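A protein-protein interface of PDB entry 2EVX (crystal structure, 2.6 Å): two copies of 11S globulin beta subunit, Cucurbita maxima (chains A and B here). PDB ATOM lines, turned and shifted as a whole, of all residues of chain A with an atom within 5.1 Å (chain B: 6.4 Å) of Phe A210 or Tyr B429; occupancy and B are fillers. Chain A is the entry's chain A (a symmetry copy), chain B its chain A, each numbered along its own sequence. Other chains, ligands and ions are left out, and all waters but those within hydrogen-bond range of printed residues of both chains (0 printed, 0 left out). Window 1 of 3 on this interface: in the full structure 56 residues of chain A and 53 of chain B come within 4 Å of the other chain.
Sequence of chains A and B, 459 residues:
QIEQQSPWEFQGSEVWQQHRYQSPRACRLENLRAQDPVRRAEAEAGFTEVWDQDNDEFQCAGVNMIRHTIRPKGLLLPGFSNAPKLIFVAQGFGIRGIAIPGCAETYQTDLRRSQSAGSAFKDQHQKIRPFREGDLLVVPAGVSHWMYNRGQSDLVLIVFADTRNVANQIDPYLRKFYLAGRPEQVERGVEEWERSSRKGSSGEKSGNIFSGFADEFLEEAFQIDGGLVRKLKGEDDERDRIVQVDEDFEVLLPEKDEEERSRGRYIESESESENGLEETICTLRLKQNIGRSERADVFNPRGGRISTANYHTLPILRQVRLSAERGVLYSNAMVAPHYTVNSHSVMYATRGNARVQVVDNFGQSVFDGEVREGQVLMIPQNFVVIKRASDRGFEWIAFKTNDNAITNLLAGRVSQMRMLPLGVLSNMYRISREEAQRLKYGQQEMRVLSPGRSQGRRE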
ATOM      1  N   LEU A 179     -25.149 -21.260  18.543  1.00  0.00           N
ATOM      2  CA  LEU A 179     -24.771 -20.210  19.486  1.00  0.00           C
ATOM      3  C   LEU A 179     -23.342 -19.695  19.304  1.00  0.00           C
ATOM      4  O   LEU A 179     -23.036 -18.536  19.631  1.00  0.00           O
ATOM      5  CB  LEU A 179     -24.963 -20.702  20.923  1.00  0.00           C
ATOM      6  CG  LEU A 179     -26.390 -21.055  21.347  1.00  0.00           C
ATOM      7  CD1 LEU A 179     -26.452 -21.230  22.851  1.00  0.00           C
ATOM      8  CD2 LEU A 179     -27.328 -19.956  20.935  1.00  0.00           C
ATOM      9  N   ALA A 180     -22.472 -20.556  18.777  1.00  0.00           N
ATOM     10  CA  ALA A 180     -21.077 -20.196  18.547  1.00  0.00           C
ATOM     11  C   ALA A 180     -20.574 -20.774  17.235  1.00  0.00           C
ATOM     12  O   ALA A 180     -21.168 -21.698  16.685  1.00  0.00           O
ATOM     13  CB  ALA A 180     -20.201 -20.697  19.704  1.00  0.00           C
ATOM     14  N   ASN A 208     -23.504 -17.595  13.254  1.00  0.00           N
ATOM     15  CA  ASN A 208     -24.243 -18.010  14.442  1.00  0.00           C
ATOM     16  C   ASN A 208     -25.226 -16.898  14.766  1.00  0.00           C
ATOM     17  O   ASN A 208     -25.108 -15.812  14.226  1.00  0.00           O
ATOM     18  CB  ASN A 208     -23.298 -18.285  15.630  1.00  0.00           C
ATOM     19  CG  ASN A 208     -22.469 -17.069  16.035  1.00  0.00           C
ATOM     20  OD1 ASN A 208     -22.978 -15.944  16.149  1.00  0.00           O
ATOM     21  ND2 ASN A 208     -21.183 -17.299  16.278  1.00  0.00           N
ATOM     22  N   ILE A 209     -26.188 -17.158  15.640  1.00  0.00           N
ATOM     23  CA  ILE A 209     -27.205 -16.157  15.967  1.00  0.00           C
ATOM     24  C   ILE A 209     -26.705 -14.767  16.367  1.00  0.00           C
ATOM     25  O   ILE A 209     -27.443 -13.793  16.268  1.00  0.00           O
ATOM     26  CB  ILE A 209     -28.131 -16.655  17.087  1.00  0.00           C
ATOM     27  CG1 ILE A 209     -27.315 -16.850  18.364  1.00  0.00           C
ATOM     28  CG2 ILE A 209     -28.803 -17.953  16.678  1.00  0.00           C
ATOM     29  CD1 ILE A 209     -28.151 -17.192  19.555  1.00  0.00           C
ATOM     30  N   PHE A 210     -25.463 -14.661  16.813  1.00  0.00           N
ATOM     31  CA  PHE A 210     -24.955 -13.359  17.224  1.00  0.00           C
ATOM     32  C   PHE A 210     -24.413 -12.479  16.099  1.00  0.00           C
ATOM     33  O   PHE A 210     -24.480 -11.252  16.185  1.00  0.00           O
ATOM     34  CB  PHE A 210     -23.873 -13.532  18.290  1.00  0.00           C
ATOM     35  CG  PHE A 210     -24.372 -14.156  19.552  1.00  0.00           C
ATOM     36  CD1 PHE A 210     -24.046 -15.474  19.872  1.00  0.00           C
ATOM     37  CD2 PHE A 210     -25.219 -13.446  20.404  1.00  0.00           C
ATOM     38  CE1 PHE A 210     -24.560 -16.080  21.021  1.00  0.00           C
ATOM     39  CE2 PHE A 210     -25.740 -14.044  21.556  1.00  0.00           C
ATOM     40  CZ  PHE A 210     -25.410 -15.363  21.863  1.00  0.00           C
ATOM     41  N   SER A 211     -23.888 -13.098  15.044  1.00  0.00           N
ATOM     42  CA  SER A 211     -23.303 -12.335  13.947  1.00  0.00           C
ATOM     43  C   SER A 211     -24.263 -11.431  13.180  1.00  0.00           C
ATOM     44  O   SER A 211     -23.828 -10.575  12.405  1.00  0.00           O
ATOM     45  CB  SER A 211     -22.542 -13.267  12.997  1.00  0.00           C
ATOM     46  OG  SER A 211     -23.315 -14.375  12.584  1.00  0.00           O
ATOM     47  N   GLY A 212     -25.564 -11.602  13.416  1.00  0.00           N
ATOM     48  CA  GLY A 212     -26.560 -10.757  12.773  1.00  0.00           C
ATOM     49  C   GLY A 212     -26.869  -9.523  13.620  1.00  0.00           C
ATOM     50  O   GLY A 212     -27.600  -8.629  13.193  1.00  0.00           O
ATOM     51  N   PHE A 213     -26.307  -9.467  14.827  1.00  0.00           N
ATOM     52  CA  PHE A 213     -26.531  -8.343  15.733  1.00  0.00           C
ATOM     53  C   PHE A 213     -25.430  -7.293  15.736  1.00  0.00           C
ATOM     54  O   PHE A 213     -24.250  -7.600  15.547  1.00  0.00           O
ATOM     55  CB  PHE A 213     -26.729  -8.846  17.168  1.00  0.00           C
ATOM     56  CG  PHE A 213     -28.070  -9.480  17.407  1.00  0.00           C
ATOM     57  CD1 PHE A 213     -29.240  -8.756  17.198  1.00  0.00           C
ATOM     58  CD2 PHE A 213     -28.165 -10.801  17.814  1.00  0.00           C
ATOM     59  CE1 PHE A 213     -30.474  -9.334  17.387  1.00  0.00           C
ATOM     60  CE2 PHE A 213     -29.395 -11.386  18.006  1.00  0.00           C
ATOM     61  CZ  PHE A 213     -30.552 -10.650  17.791  1.00  0.00           C
ATOM     62  N   LEU A 218     -24.790  -6.035  21.377  1.00  0.00           N
ATOM     63  CA  LEU A 218     -24.221  -7.180  22.068  1.00  0.00           C
ATOM     64  C   LEU A 218     -23.318  -6.815  23.231  1.00  0.00           C
ATOM     65  O   LEU A 218     -23.197  -7.585  24.182  1.00  0.00           O
ATOM     66  CB  LEU A 218     -23.456  -8.076  21.095  1.00  0.00           C
ATOM     67  CG  LEU A 218     -24.275  -8.822  20.038  1.00  0.00           C
ATOM     68  CD1 LEU A 218     -23.345  -9.748  19.285  1.00  0.00           C
ATOM     69  CD2 LEU A 218     -25.411  -9.625  20.680  1.00  0.00           C
ATOM     70  N   PHE A 222     -24.570  -8.240  27.121  1.00  0.00           N
ATOM     71  CA  PHE A 222     -23.634  -9.055  27.879  1.00  0.00           C
ATOM     72  C   PHE A 222     -22.712  -8.267  28.793  1.00  0.00           C
ATOM     73  O   PHE A 222     -22.108  -8.842  29.697  1.00  0.00           O
ATOM     74  CB  PHE A 222     -22.773  -9.899  26.937  1.00  0.00           C
ATOM     75  CG  PHE A 222     -23.555 -10.835  26.076  1.00  0.00           C
ATOM     76  CD1 PHE A 222     -24.257 -10.364  24.975  1.00  0.00           C
ATOM     77  CD2 PHE A 222     -23.591 -12.193  26.366  1.00  0.00           C
ATOM     78  CE1 PHE A 222     -24.980 -11.229  24.176  1.00  0.00           C
ATOM     79  CE2 PHE A 222     -24.317 -13.069  25.567  1.00  0.00           C
ATOM     80  CZ  PHE A 222     -25.010 -12.586  24.472  1.00  0.00           C
ATOM     81  N   LYS A 231     -15.311 -12.237  19.138  1.00  0.00           N
ATOM     82  CA  LYS A 231     -15.210 -13.670  19.373  1.00  0.00           C
ATOM     83  C   LYS A 231     -16.602 -14.290  19.326  1.00  0.00           C
ATOM     84  O   LYS A 231     -16.824 -15.318  18.693  1.00  0.00           O
ATOM     85  CB  LYS A 231     -14.595 -13.923  20.744  1.00  0.00           C
ATOM     86  CG  LYS A 231     -13.198 -13.394  20.893  1.00  0.00           C
ATOM     87  CD  LYS A 231     -12.198 -14.414  20.425  1.00  0.00           C
ATOM     88  CE  LYS A 231     -10.823 -14.039  20.915  1.00  0.00           C
ATOM     89  NZ  LYS A 231      -9.919 -15.218  20.939  1.00  0.00           N
ATOM     90  N   LEU A 232     -17.532 -13.648  20.015  1.00  0.00           N
ATOM     91  CA  LEU A 232     -18.903 -14.104  20.079  1.00  0.00           C
ATOM     92  C   LEU A 232     -19.420 -14.322  18.661  1.00  0.00           C
ATOM     93  O   LEU A 232     -19.846 -15.419  18.306  1.00  0.00           O
ATOM     94  CB  LEU A 232     -19.743 -13.054  20.804  1.00  0.00           C
ATOM     95  CG  LEU A 232     -21.142 -13.426  21.299  1.00  0.00           C
ATOM     96  CD1 LEU A 232     -21.072 -14.592  22.302  1.00  0.00           C
ATOM     97  CD2 LEU A 232     -21.769 -12.186  21.938  1.00  0.00           C
ATOM     98  N   LYS A 233     -19.364 -13.270  17.850  1.00  0.00           N
ATOM     99  CA  LYS A 233     -19.822 -13.351  16.473  1.00  0.00           C
ATOM    100  C   LYS A 233     -19.056 -14.398  15.678  1.00  0.00           C
ATOM    101  O   LYS A 233     -19.494 -14.818  14.605  1.00  0.00           O
ATOM    102  CB  LYS A 233     -19.675 -11.998  15.781  1.00  0.00           C
ATOM    103  CG  LYS A 233     -20.547 -10.891  16.339  1.00  0.00           C
ATOM    104  CD  LYS A 233     -20.526  -9.710  15.392  1.00  0.00           C
ATOM    105  CE  LYS A 233     -21.474  -8.614  15.811  1.00  0.00           C
ATOM    106  NZ  LYS A 233     -21.489  -7.544  14.786  1.00  0.00           N
ATOM    107  N   ARG A 239     -13.802 -23.373  11.748  1.00  0.00           N
ATOM    108  CA  ARG A 239     -13.852 -24.759  12.200  1.00  0.00           C
ATOM    109  C   ARG A 239     -15.143 -25.505  11.876  1.00  0.00           C
ATOM    110  O   ARG A 239     -15.184 -26.733  11.914  1.00  0.00           O
ATOM    111  CB  ARG A 239     -13.626 -24.791  13.707  1.00  0.00           C
ATOM    112  CG  ARG A 239     -12.362 -24.089  14.124  1.00  0.00           C
ATOM    113  CD  ARG A 239     -12.250 -24.024  15.610  1.00  0.00           C
ATOM    114  NE  ARG A 239     -13.248 -23.132  16.173  1.00  0.00           N
ATOM    115  CZ  ARG A 239     -13.632 -23.173  17.443  1.00  0.00           C
ATOM    116  NH1 ARG A 239     -14.551 -22.327  17.889  1.00  0.00           N
ATOM    117  NH2 ARG A 239     -13.097 -24.075  18.262  1.00  0.00           N
ATOM    118  N   PRO B 337     -31.324 -10.134  24.531  1.00  0.00           N
ATOM    119  CA  PRO B 337     -31.509 -11.043  23.399  1.00  0.00           C
ATOM    120  C   PRO B 337     -32.232 -12.305  23.841  1.00  0.00           C
ATOM    121  O   PRO B 337     -32.014 -12.813  24.938  1.00  0.00           O
ATOM    122  CB  PRO B 337     -30.079 -11.309  22.920  1.00  0.00           C
ATOM    123  CG  PRO B 337     -29.239 -10.983  24.101  1.00  0.00           C
ATOM    124  CD  PRO B 337     -29.906  -9.772  24.669  1.00  0.00           C
ATOM    125  N   VAL B 359     -32.708 -11.832  14.116  1.00  0.00           N
ATOM    126  CA  VAL B 359     -31.721 -12.619  13.390  1.00  0.00           C
ATOM    127  C   VAL B 359     -32.279 -14.029  13.177  1.00  0.00           C
ATOM    128  O   VAL B 359     -32.992 -14.556  14.036  1.00  0.00           O
ATOM    129  CB  VAL B 359     -30.394 -12.723  14.189  1.00  0.00           C
ATOM    130  CG1 VAL B 359     -29.438 -13.668  13.493  1.00  0.00           C
ATOM    131  CG2 VAL B 359     -29.756 -11.347  14.330  1.00  0.00           C
ATOM    132  N   GLY B 363     -27.827 -16.663  10.876  1.00  0.00           N
ATOM    133  CA  GLY B 363     -27.016 -15.665  11.536  1.00  0.00           C
ATOM    134  C   GLY B 363     -27.160 -14.351  10.813  1.00  0.00           C
ATOM    135  O   GLY B 363     -26.370 -13.425  11.012  1.00  0.00           O
ATOM    136  N   VAL B 384     -33.937 -15.061  17.060  1.00  0.00           N
ATOM    137  CA  VAL B 384     -33.402 -14.311  18.177  1.00  0.00           C
ATOM    138  C   VAL B 384     -33.752 -12.862  17.937  1.00  0.00           C
ATOM    139  O   VAL B 384     -33.832 -12.421  16.794  1.00  0.00           O
ATOM    140  CB  VAL B 384     -31.874 -14.480  18.294  1.00  0.00           C
ATOM    141  CG1 VAL B 384     -31.384 -13.830  19.570  1.00  0.00           C
ATOM    142  CG2 VAL B 384     -31.507 -15.961  18.284  1.00  0.00           C
ATOM    143  N   LEU B 410     -30.545 -15.312  26.332  1.00  0.00           N
ATOM    144  CA  LEU B 410     -29.208 -15.561  25.852  1.00  0.00           C
ATOM    145  C   LEU B 410     -28.187 -14.974  26.810  1.00  0.00           C
ATOM    146  O   LEU B 410     -27.110 -15.550  27.000  1.00  0.00           O
ATOM    147  CB  LEU B 410     -29.040 -14.995  24.443  1.00  0.00           C
ATOM    148  CG  LEU B 410     -29.294 -15.984  23.294  1.00  0.00           C
ATOM    149  CD1 LEU B 410     -29.949 -17.265  23.801  1.00  0.00           C
ATOM    150  CD2 LEU B 410     -30.157 -15.307  22.241  1.00  0.00           C
ATOM    151  N   MET B 417     -26.346 -18.893  28.326  1.00  0.00           N
ATOM    152  CA  MET B 417     -24.943 -18.713  28.663  1.00  0.00           C
ATOM    153  C   MET B 417     -24.620 -19.261  30.054  1.00  0.00           C
ATOM    154  O   MET B 417     -23.670 -20.026  30.218  1.00  0.00           O
ATOM    155  CB  MET B 417     -24.582 -17.228  28.584  1.00  0.00           C
ATOM    156  CG  MET B 417     -23.112 -16.952  28.275  1.00  0.00           C
ATOM    157  SD  MET B 417     -22.608 -17.417  26.583  1.00  0.00           S
ATOM    158  CE  MET B 417     -23.183 -15.969  25.682  1.00  0.00           C
ATOM    159  N   LEU B 420     -24.156 -22.904  30.418  1.00  0.00           N
ATOM    160  CA  LEU B 420     -22.966 -23.487  29.818  1.00  0.00           C
ATOM    161  C   LEU B 420     -21.709 -23.532  30.676  1.00  0.00           C
ATOM    162  O   LEU B 420     -21.384 -22.568  31.365  1.00  0.00           O
ATOM    163  CB  LEU B 420     -22.668 -22.770  28.496  1.00  0.00           C
ATOM    164  CG  LEU B 420     -23.728 -22.958  27.393  1.00  0.00           C
ATOM    165  CD1 LEU B 420     -23.496 -21.961  26.266  1.00  0.00           C
ATOM    166  CD2 LEU B 420     -23.695 -24.401  26.883  1.00  0.00           C
ATOM    167  N   VAL B 424     -16.688 -25.335  27.953  1.00  0.00           N
ATOM    168  CA  VAL B 424     -17.370 -25.333  26.665  1.00  0.00           C
ATOM    169  C   VAL B 424     -17.396 -23.931  26.051  1.00  0.00           C
ATOM    170  O   VAL B 424     -17.086 -23.757  24.875  1.00  0.00           O
ATOM    171  CB  VAL B 424     -18.814 -25.883  26.815  1.00  0.00           C
ATOM    172  CG1 VAL B 424     -19.569 -25.771  25.502  1.00  0.00           C
ATOM    173  CG2 VAL B 424     -18.763 -27.338  27.253  1.00  0.00           C
ATOM    174  N   LEU B 425     -17.758 -22.926  26.838  1.00  0.00           N
ATOM    175  CA  LEU B 425     -17.790 -21.561  26.322  1.00  0.00           C
ATOM    176  C   LEU B 425     -16.431 -21.186  25.737  1.00  0.00           C
ATOM    177  O   LEU B 425     -16.354 -20.477  24.728  1.00  0.00           O
ATOM    178  CB  LEU B 425     -18.137 -20.567  27.426  1.00  0.00           C
ATOM    179  CG  LEU B 425     -19.513 -20.617  28.085  1.00  0.00           C
ATOM    180  CD1 LEU B 425     -19.613 -19.472  29.075  1.00  0.00           C
ATOM    181  CD2 LEU B 425     -20.602 -20.488  27.046  1.00  0.00           C
ATOM    182  N   SER B 426     -15.363 -21.661  26.375  1.00  0.00           N
ATOM    183  CA  SER B 426     -14.001 -21.369  25.929  1.00  0.00           C
ATOM    184  C   SER B 426     -13.747 -21.813  24.499  1.00  0.00           C
ATOM    185  O   SER B 426     -13.387 -21.013  23.630  1.00  0.00           O
ATOM    186  CB  SER B 426     -12.983 -22.054  26.840  1.00  0.00           C
ATOM    187  OG  SER B 426     -12.715 -21.264  27.982  1.00  0.00           O
ATOM    188  N   ASN B 427     -13.919 -23.108  24.274  1.00  0.00           N
ATOM    189  CA  ASN B 427     -13.715 -23.681  22.965  1.00  0.00           C
ATOM    190  C   ASN B 427     -14.717 -23.120  21.955  1.00  0.00           C
ATOM    191  O   ASN B 427     -14.432 -23.063  20.760  1.00  0.00           O
ATOM    192  CB  ASN B 427     -13.820 -25.197  23.071  1.00  0.00           C
ATOM    193  CG  ASN B 427     -12.651 -25.800  23.825  1.00  0.00           C
ATOM    194  OD1 ASN B 427     -11.563 -25.969  23.275  1.00  0.00           O
ATOM    195  ND2 ASN B 427     -12.867 -26.115  25.096  1.00  0.00           N
ATOM    196  N   MET B 428     -15.883 -22.695  22.438  1.00  0.00           N
ATOM    197  CA  MET B 428     -16.914 -22.132  21.571  1.00  0.00           C
ATOM    198  C   MET B 428     -16.470 -20.817  20.935  1.00  0.00           C
ATOM    199  O   MET B 428     -16.554 -20.642  19.719  1.00  0.00           O
ATOM    200  CB  MET B 428     -18.216 -21.898  22.359  1.00  0.00           C
ATOM    201  CG  MET B 428     -19.082 -23.148  22.569  1.00  0.00           C
ATOM    202  SD  MET B 428     -20.526 -22.893  23.675  1.00  0.00           S
ATOM    203  CE  MET B 428     -21.511 -21.693  22.741  1.00  0.00           C
ATOM    204  N   TYR B 429     -15.988 -19.890  21.754  1.00  0.00           N
ATOM    205  CA  TYR B 429     -15.575 -18.596  21.232  1.00  0.00           C
ATOM    206  C   TYR B 429     -14.072 -18.353  21.220  1.00  0.00           C
ATOM    207  O   TYR B 429     -13.615 -17.209  21.190  1.00  0.00           O
ATOM    208  CB  TYR B 429     -16.286 -17.501  22.016  1.00  0.00           C
ATOM    209  CG  TYR B 429     -17.774 -17.718  22.064  1.00  0.00           C
ATOM    210  CD1 TYR B 429     -18.355 -18.499  23.063  1.00  0.00           C
ATOM    211  CD2 TYR B 429     -18.604 -17.166  21.094  1.00  0.00           C
ATOM    212  CE1 TYR B 429     -19.728 -18.720  23.098  1.00  0.00           C
ATOM    213  CE2 TYR B 429     -19.975 -17.380  21.114  1.00  0.00           C
ATOM    214  CZ  TYR B 429     -20.532 -18.155  22.116  1.00  0.00           C
ATOM    215  OH  TYR B 429     -21.894 -18.350  22.137  1.00  0.00           O
ATOM    216  N   ARG B 430     -13.312 -19.441  21.220  1.00  0.00           N
ATOM    217  CA  ARG B 430     -11.857 -19.380  21.214  1.00  0.00           C
ATOM    218  C   ARG B 430     -11.358 -18.297  22.159  1.00  0.00           C
ATOM    219  O   ARG B 430     -10.406 -17.587  21.855  1.00  0.00           O
ATOM    220  CB  ARG B 430     -11.328 -19.114  19.799  1.00  0.00           C
ATOM    221  CG  ARG B 430     -11.769 -20.130  18.753  1.00  0.00           C
ATOM    222  CD  ARG B 430     -12.693 -19.475  17.747  1.00  0.00           C
ATOM    223  NE  ARG B 430     -11.998 -18.480  16.934  1.00  0.00           N
ATOM    224  CZ  ARG B 430     -12.600 -17.472  16.305  1.00  0.00           C
ATOM    225  NH1 ARG B 430     -13.917 -17.322  16.400  1.00  0.00           N
ATOM    226  NH2 ARG B 430     -11.888 -16.612  15.584  1.00  0.00           N
ATOM    227  N   ILE B 431     -12.025 -18.163  23.300  1.00  0.00           N
ATOM    228  CA  ILE B 431     -11.630 -17.187  24.304  1.00  0.00           C
ATOM    229  C   ILE B 431     -11.062 -17.962  25.478  1.00  0.00           C
ATOM    230  O   ILE B 431     -11.009 -19.188  25.448  1.00  0.00           O
ATOM    231  CB  ILE B 431     -12.823 -16.360  24.792  1.00  0.00           C
ATOM    232  CG1 ILE B 431     -13.901 -17.293  25.343  1.00  0.00           C
ATOM    233  CG2 ILE B 431     -13.343 -15.482  23.656  1.00  0.00           C
ATOM    234  CD1 ILE B 431     -15.158 -16.593  25.746  1.00  0.00           C
ATOM    235  N   SER B 432     -10.633 -17.251  26.508  1.00  0.00           N
ATOM    236  CA  SER B 432     -10.062 -17.899  27.682  1.00  0.00           C
ATOM    237  C   SER B 432     -11.102 -18.070  28.778  1.00  0.00           C
ATOM    238  O   SER B 432     -12.075 -17.315  28.854  1.00  0.00           O
ATOM    239  CB  SER B 432      -8.912 -17.067  28.228  1.00  0.00           C
ATOM    240  OG  SER B 432      -9.407 -15.828  28.702  1.00  0.00           O
ATOM    241  N   LEU B 439     -18.118 -13.343  30.252  1.00  0.00           N
ATOM    242  CA  LEU B 439     -19.192 -13.530  29.285  1.00  0.00           C
ATOM    243  C   LEU B 439     -20.497 -13.971  29.937  1.00  0.00           C
ATOM    244  O   LEU B 439     -21.554 -13.401  29.659  1.00  0.00           O
ATOM    245  CB  LEU B 439     -18.793 -14.566  28.233  1.00  0.00           C
ATOM    246  CG  LEU B 439     -19.090 -14.210  26.773  1.00  0.00           C
ATOM    247  CD1 LEU B 439     -19.129 -15.494  25.957  1.00  0.00           C
ATOM    248  CD2 LEU B 439     -20.408 -13.460  26.662  1.00  0.00           C
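The backbone carbonyl oxygen of Gly B363 sits at hydrogen-bond distance from the backbone NH of Gly A212, 3.1 Å away.
O of Asn B427 sits at hydrogen-bond distance from NH1 of Arg A239 (3.0 Å).
O of Met B428 is in hydrogen-bond range of NH1 of Arg A239 (3.2 Å).
The side-chain hydroxyl (OH) of Tyr B429 sits at hydrogen-bond distance from the backbone carbonyl oxygen (O) of Leu A179 (2.8 Å).
O of Arg B430 is in hydrogen-bond range of NZ of Lys A231 (2.6 Å).
The backbone carbonyl oxygen (O) of Pro B337 is in hydrogen-bond range of the backbone NH (N) of Leu B410.
O of Val B384 is in hydrogen-bond range of N of Val B359, 3.0 Å away.
The backbone carbonyl oxygen (O) of Ser B426 is in hydrogen-bond range of the backbone NH (N) of Ile B431 (3.2 Å).
N of Phe A210 is in hydrogen-bond range of OD1 of Asn A208, at 2.9 Å.
The side-chain hydroxyl of Ser A211 lies within hydrogen-bond range of the backbone carbonyl oxygen of Asn A208 (2.8 Å).
ND2 of Asn A208 lies within hydrogen-bond range of O of Leu A232.
CE of Met B428 touches CB of Ala A180 (3.5 Å).
CZ of Tyr B429 touches CB of Ala A180 (3.5 Å).
Val B359 touches Ile A209.
CB of Ile A209 touches CG2 of Val B384 (3.6 Å).
OH of Tyr B429 touches CE1 of Phe A210, 3.7 Å away.
Phe A213 touches Val B384.
Met B417 touches Phe A222 (CE to CE2, 3.1 Å).
O of Tyr B429 touches CD of Lys A231, at 3.2 Å.
Leu A232 touches Tyr B429 (CD1 to CE2, 3.2 Å).
CD of Arg B430 touches NH1 of Arg A239 (3.4 Å).
Printed residues of chain B within 4 Å of Ala A180: Met B428 and Tyr B429.
Printed residues of chain A within 4 Å of Val B384: Ile A209 and Phe A213.
Val B424 touches none of the printed residues of chain A.
Of the printed residues of chain A, Asn B427 touches Arg A239 (3.0 Å).
Tyr B429 touches just these residues of chain A: Leu A179 (2.8 Å), Ala A180 (3.5 Å), Phe A210 (3.7 Å), Lys A231 (3.2 Å) and Leu A232 (3.2 Å).
Of the printed residues of chain A, Leu B439 touches Phe A222.
The nearest residue of chain B that does not touch Phe A210 is Leu B410 (4.2 Å).
The nearest printed residue of chain A that does not touch Met B428 is Leu A179 (4.03 Å).
Hydrophobic or aromatic side chains of chain B within 4 Å of the printed part of chain A: Val B359, Val B384, Leu B410, Met B417, Met B428, Tyr B429, Ile B431 and Leu B439.
Hydrophobic or aromatic side chains of chain A that line the printed part of chain B: Ala A180, Ile A209, Phe A210, Phe A213, Phe A222 and Leu A232.
Among the printed residues, 22 pairs touch across the chains.
No position is printed for both chains.
Of the 22 pairs that touch across the chains among the printed residues, none has its exchanged pair printed and touching as well.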
